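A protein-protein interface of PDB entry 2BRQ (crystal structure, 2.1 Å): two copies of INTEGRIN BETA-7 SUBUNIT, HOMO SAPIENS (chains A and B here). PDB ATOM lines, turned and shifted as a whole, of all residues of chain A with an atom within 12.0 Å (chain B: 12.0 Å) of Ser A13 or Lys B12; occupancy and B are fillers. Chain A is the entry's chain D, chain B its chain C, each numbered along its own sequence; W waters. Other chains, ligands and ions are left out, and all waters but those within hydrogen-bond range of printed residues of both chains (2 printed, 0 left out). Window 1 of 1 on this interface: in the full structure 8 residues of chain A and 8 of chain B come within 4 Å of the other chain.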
ATOM      1  N   PRO A   9      19.413 -15.475  -6.371  1.00  0.00           N
ATOM      2  CA  PRO A   9      19.348 -16.047  -4.995  1.00  0.00           C
ATOM      3  C   PRO A   9      20.705 -16.418  -4.417  1.00  0.00           C
ATOM      4  O   PRO A   9      21.637 -16.689  -5.155  1.00  0.00           O
ATOM      5  CB  PRO A   9      18.487 -17.313  -5.146  1.00  0.00           C
ATOM      6  CG  PRO A   9      17.799 -17.162  -6.472  1.00  0.00           C
ATOM      7  CD  PRO A   9      18.731 -16.332  -7.349  1.00  0.00           C
ATOM      8  N   LEU A  10      20.812 -16.399  -3.095  1.00  0.00           N
ATOM      9  CA  LEU A  10      21.995 -16.924  -2.415  1.00  0.00           C
ATOM     10  C   LEU A  10      21.601 -18.268  -1.779  1.00  0.00           C
ATOM     11  O   LEU A  10      20.583 -18.376  -1.110  1.00  0.00           O
ATOM     12  CB  LEU A  10      22.460 -15.927  -1.324  1.00  0.00           C
ATOM     13  CG  LEU A  10      23.708 -16.257  -0.485  1.00  0.00           C
ATOM     14  CD1 LEU A  10      24.956 -16.179  -1.331  1.00  0.00           C
ATOM     15  CD2 LEU A  10      23.826 -15.303   0.662  1.00  0.00           C
ATOM     16  N   TYR A  11      22.440 -19.271  -1.979  1.00  0.00           N
ATOM     17  CA  TYR A  11      22.172 -20.613  -1.535  1.00  0.00           C
ATOM     18  C   TYR A  11      23.162 -20.958  -0.437  1.00  0.00           C
ATOM     19  O   TYR A  11      24.297 -20.518  -0.484  1.00  0.00           O
ATOM     20  CB  TYR A  11      22.349 -21.569  -2.708  1.00  0.00           C
ATOM     21  CG  TYR A  11      21.300 -21.417  -3.778  1.00  0.00           C
ATOM     22  CD1 TYR A  11      21.453 -20.506  -4.833  1.00  0.00           C
ATOM     23  CD2 TYR A  11      20.163 -22.198  -3.747  1.00  0.00           C
ATOM     24  CE1 TYR A  11      20.454 -20.384  -5.839  1.00  0.00           C
ATOM     25  CE2 TYR A  11      19.191 -22.083  -4.694  1.00  0.00           C
ATOM     26  CZ  TYR A  11      19.338 -21.178  -5.748  1.00  0.00           C
ATOM     27  OH  TYR A  11      18.320 -21.112  -6.680  1.00  0.00           O
ATOM     28  N   LYS A  12      22.720 -21.715   0.569  1.00  0.00           N
ATOM     29  CA  LYS A  12      23.641 -22.276   1.557  1.00  0.00           C
ATOM     30  C   LYS A  12      23.288 -23.749   1.781  1.00  0.00           C
ATOM     31  O   LYS A  12      22.116 -24.079   1.868  1.00  0.00           O
ATOM     32  CB  LYS A  12      23.572 -21.512   2.896  1.00  0.00           C
ATOM     33  CG  LYS A  12      24.753 -21.821   3.809  1.00  0.00           C
ATOM     34  CD  LYS A  12      24.709 -20.973   5.081  1.00  0.00           C
ATOM     35  CE  LYS A  12      26.092 -21.028   5.736  1.00  0.00           C
ATOM     36  NZ  LYS A  12      26.324 -19.978   6.766  1.00  0.00           N
ATOM     37  N   SER A  13      24.305 -24.611   1.801  1.00  0.00           N
ATOM     38  CA  SER A  13      24.139 -25.999   2.211  1.00  0.00           C
ATOM     39  C   SER A  13      25.100 -26.218   3.360  1.00  0.00           C
ATOM     40  O   SER A  13      26.217 -25.733   3.318  1.00  0.00           O
ATOM     41  CB  SER A  13      24.504 -26.980   1.094  1.00  0.00           C
ATOM     42  OG  SER A  13      23.565 -26.919   0.036  1.00  0.00           O
ATOM     43  N   ALA A  14      24.678 -26.982   4.353  1.00  0.00           N
ATOM     44  CA  ALA A  14      25.543 -27.296   5.512  1.00  0.00           C
ATOM     45  C   ALA A  14      25.293 -28.728   5.973  1.00  0.00           C
ATOM     46  O   ALA A  14      24.184 -29.287   5.846  1.00  0.00           O
ATOM     47  CB  ALA A  14      25.306 -26.322   6.670  1.00  0.00           C
ATOM     48  N   ILE A  15      26.355 -29.312   6.511  1.00  0.00           N
ATOM     49  CA  ILE A  15      26.278 -30.651   7.026  1.00  0.00           C
ATOM     50  C   ILE A  15      27.086 -30.642   8.317  1.00  0.00           C
ATOM     51  O   ILE A  15      28.227 -30.135   8.353  1.00  0.00           O
ATOM     52  CB  ILE A  15      26.773 -31.651   5.941  1.00  0.00           C
ATOM     53  CG1 ILE A  15      26.556 -33.105   6.348  1.00  0.00           C
ATOM     54  CG2 ILE A  15      28.245 -31.366   5.540  1.00  0.00           C
ATOM     55  CD1 ILE A  15      26.830 -34.020   5.164  1.00  0.00           C
ATOM     56  N   THR A  16      26.464 -31.129   9.382  1.00  0.00           N
ATOM     57  CA  THR A  16      27.109 -31.216  10.686  1.00  0.00           C
ATOM     58  C   THR A  16      27.198 -32.680  11.138  1.00  0.00           C
ATOM     59  O   THR A  16      26.191 -33.372  11.190  1.00  0.00           O
ATOM     60  CB  THR A  16      26.347 -30.405  11.734  1.00  0.00           C
ATOM     61  OG1 THR A  16      26.175 -29.050  11.282  1.00  0.00           O
ATOM     62  CG2 THR A  16      27.065 -30.441  13.066  1.00  0.00           C
ATOM     63  N   THR A  17      28.407 -33.150  11.443  1.00  0.00           N
ATOM     64  CA  THR A  17      28.574 -34.461  12.071  1.00  0.00           C
ATOM     65  C   THR A  17      29.134 -34.316  13.495  1.00  0.00           C
ATOM     66  O   THR A  17      29.878 -33.388  13.788  1.00  0.00           O
ATOM     67  CB  THR A  17      29.453 -35.416  11.193  1.00  0.00           C
ATOM     68  OG1 THR A  17      29.300 -36.781  11.626  1.00  0.00           O
ATOM     69  CG2 THR A  17      30.944 -35.040  11.253  1.00  0.00           C
ATOM     70  N   PRO B   9      24.040 -37.497  10.172  1.00  0.00           N
ATOM     71  CA  PRO B   9      24.379 -36.070  10.200  1.00  0.00           C
ATOM     72  C   PRO B   9      23.174 -35.149  10.355  1.00  0.00           C
ATOM     73  O   PRO B   9      22.016 -35.573  10.165  1.00  0.00           O
ATOM     74  CB  PRO B   9      25.035 -35.833   8.832  1.00  0.00           C
ATOM     75  CG  PRO B   9      25.603 -37.143   8.448  1.00  0.00           C
ATOM     76  CD  PRO B   9      24.628 -38.180   9.004  1.00  0.00           C
ATOM     77  N   LEU B  10      23.449 -33.898  10.717  1.00  0.00           N
ATOM     78  CA  LEU B  10      22.428 -32.852  10.689  1.00  0.00           C
ATOM     79  C   LEU B  10      22.612 -31.923   9.459  1.00  0.00           C
ATOM     80  O   LEU B  10      23.715 -31.385   9.233  1.00  0.00           O
ATOM     81  CB  LEU B  10      22.464 -32.065  12.005  1.00  0.00           C
ATOM     82  CG  LEU B  10      21.433 -30.948  12.183  1.00  0.00           C
ATOM     83  CD1 LEU B  10      20.026 -31.524  12.295  1.00  0.00           C
ATOM     84  CD2 LEU B  10      21.800 -30.166  13.427  1.00  0.00           C
ATOM     85  N   TYR B  11      21.544 -31.766   8.669  1.00  0.00           N
ATOM     86  CA  TYR B  11      21.605 -31.083   7.378  1.00  0.00           C
ATOM     87  C   TYR B  11      20.859 -29.763   7.399  1.00  0.00           C
ATOM     88  O   TYR B  11      19.764 -29.671   7.929  1.00  0.00           O
ATOM     89  CB  TYR B  11      21.019 -31.958   6.271  1.00  0.00           C
ATOM     90  CG  TYR B  11      21.817 -33.207   5.969  1.00  0.00           C
ATOM     91  CD1 TYR B  11      21.588 -34.385   6.667  1.00  0.00           C
ATOM     92  CD2 TYR B  11      22.799 -33.206   4.983  1.00  0.00           C
ATOM     93  CE1 TYR B  11      22.313 -35.539   6.393  1.00  0.00           C
ATOM     94  CE2 TYR B  11      23.530 -34.354   4.694  1.00  0.00           C
ATOM     95  CZ  TYR B  11      23.280 -35.520   5.401  1.00  0.00           C
ATOM     96  OH  TYR B  11      24.009 -36.667   5.118  1.00  0.00           O
ATOM     97  N   LYS B  12      21.450 -28.728   6.840  1.00  0.00           N
ATOM     98  CA  LYS B  12      20.692 -27.495   6.671  1.00  0.00           C
ATOM     99  C   LYS B  12      20.811 -27.027   5.226  1.00  0.00           C
ATOM    100  O   LYS B  12      21.902 -27.096   4.665  1.00  0.00           O
ATOM    101  CB  LYS B  12      21.182 -26.393   7.620  1.00  0.00           C
ATOM    102  CG  LYS B  12      20.234 -25.156   7.599  1.00  0.00           C
ATOM    103  CD  LYS B  12      20.705 -24.031   8.505  1.00  0.00           C
ATOM    104  CE  LYS B  12      19.505 -23.398   9.202  1.00  0.00           C
ATOM    105  NZ  LYS B  12      19.967 -22.371  10.182  1.00  0.00           N
ATOM    106  N   SER B  13      19.686 -26.604   4.630  1.00  0.00           N
ATOM    107  CA  SER B  13      19.681 -25.921   3.321  1.00  0.00           C
ATOM    108  C   SER B  13      18.911 -24.633   3.448  1.00  0.00           C
ATOM    109  O   SER B  13      17.898 -24.598   4.130  1.00  0.00           O
ATOM    110  CB  SER B  13      18.989 -26.756   2.238  1.00  0.00           C
ATOM    111  OG  SER B  13      19.600 -28.039   2.112  1.00  0.00           O
ATOM    112  N   ALA B  14      19.392 -23.598   2.754  1.00  0.00           N
ATOM    113  CA  ALA B  14      18.815 -22.264   2.807  1.00  0.00           C
ATOM    114  C   ALA B  14      18.858 -21.656   1.406  1.00  0.00           C
ATOM    115  O   ALA B  14      19.759 -21.913   0.611  1.00  0.00           O
ATOM    116  CB  ALA B  14      19.587 -21.357   3.798  1.00  0.00           C
ATOM    117  N   ILE B  15      17.863 -20.827   1.140  1.00  0.00           N
ATOM    118  CA  ILE B  15      17.861 -20.014  -0.074  1.00  0.00           C
ATOM    119  C   ILE B  15      17.431 -18.595   0.379  1.00  0.00           C
ATOM    120  O   ILE B  15      16.530 -18.460   1.226  1.00  0.00           O
ATOM    121  CB  ILE B  15      16.906 -20.650  -1.127  1.00  0.00           C
ATOM    122  CG1 ILE B  15      16.964 -19.877  -2.454  1.00  0.00           C
ATOM    123  CG2 ILE B  15      15.436 -20.740  -0.573  1.00  0.00           C
ATOM    124  CD1 ILE B  15      16.328 -20.686  -3.615  1.00  0.00           C
ATOM    125  N   THR B  16      18.078 -17.564  -0.158  1.00  0.00           N
ATOM    126  CA  THR B  16      17.780 -16.179   0.209  1.00  0.00           C
ATOM    127  C   THR B  16      17.582 -15.323  -1.033  1.00  0.00           C
ATOM    128  O   THR B  16      18.431 -15.286  -1.919  1.00  0.00           O
ATOM    129  CB  THR B  16      18.891 -15.573   1.096  1.00  0.00           C
ATOM    130  OG1 THR B  16      19.158 -16.468   2.198  1.00  0.00           O
ATOM    131  CG2 THR B  16      18.485 -14.177   1.646  1.00  0.00           C
HETATM  132  O   HOH W   1      20.560 -18.479   1.756  1.00  0.00           O
HETATM  133  O   HOH W   2      24.126 -28.638   9.383  1.00  0.00           O
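Leu A10 touches Thr B16, and with the chains exchanged Thr A16 touches Leu B10.
Tyr A11 touches Ala B14, and with the chains exchanged Ala A14 touches Tyr B11.
Lys A12 touches Ala B14, and with the chains exchanged Ala A14 touches Lys B12.
Ile A15 touches Pro B9, but with the chains exchanged Pro A9 does not touch Ile B15 (4.02 Å).
Of the 15 pairs that touch across the chains among the printed residues, 14 have their exchanged pair printed and touching as well.
Among the printed residues, merely in contact across the chains: Pro A9 with Thr B16 (3.3 Å), Leu A10 with Ile B15 (3.3 Å), Ile A15 with Tyr B11 (3.3 Å), Tyr A11 with Ile B15 (3.4 Å), Lys A12 with Ser B13 (3.4 Å), Thr A16 with Pro B9 (3.4 Å), Ile A15 with Leu B10 (3.5 Å), Tyr A11 with Ala B14 (3.5 Å), Ala A14 with Tyr B11 (3.5 Å), Ser A13 with Lys B12 (3.5 Å) and Ile A15 with Pro B9 (3.99 Å).
Water W1 bridges the side-chain hydroxyl of Thr B16 and the backbone carbonyl oxygen of Leu A10.
Water W2 lies within hydrogen-bond range of O of Leu B10 and OG1 of Thr A16.
Of the 8 printed residues of chain B, 8 touch a printed residue of chain A.
Printed residues of chain B that touch a printed residue of chain A: Pro B9, Leu B10, Tyr B11, Lys B12, Ser B13, Ala B14, Ile B15 and Thr B16.
Hydrophobic or aromatic side chains of chain B within 4 Å of the printed part of chain A: Pro B9, Tyr B11 and Ile B15.
Along chain B the printed residues that touch a printed residue of chain A span positions 9 to 16.
O of Leu B10 lies within hydrogen-bond range of N of Thr A16 (2.8 Å).
The backbone carbonyl oxygen (O) of Lys B12 lies within hydrogen-bond range of the backbone NH (N) of Ala A14.
O of Lys A12 lies within hydrogen-bond range of N of Ala B14, 2.9 Å away.
The backbone carbonyl oxygen (O) of Leu A10 lies within hydrogen-bond range of the backbone NH (N) of Thr B16 (2.8 Å).
Printed residues of chain B within 4 Å of Pro A9: Thr B16.
Ser A13 touches just one residue of chain B: Lys B12.
Thr A17 touches none of the printed residues of chain B.
Printed residues of chain A within 4 Å of Pro B9: Ile A15 and Thr A16.
Of chain A, only Ser A13 (3.5 Å) and Ala A14 (2.8 Å) come within 4 Å of Lys B12.
Of the printed residues of chain A, Ala B14 touches Tyr A11 (3.5 Å) and Lys A12 (2.9 Å).
Of the printed residues of chain A, Thr B16 touches Pro A9 (3.3 Å) and Leu A10 (2.8 Å).
The nearest residue of chain B that does not touch Ser A13 is Ser B13 (4.6 Å).
The nearest residue of chain A that does not touch Lys B12 is Lys A12 (4.1 Å).
The nearest printed residue of chain B that does not touch Thr A16 is Tyr B11 (5.0 Å).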
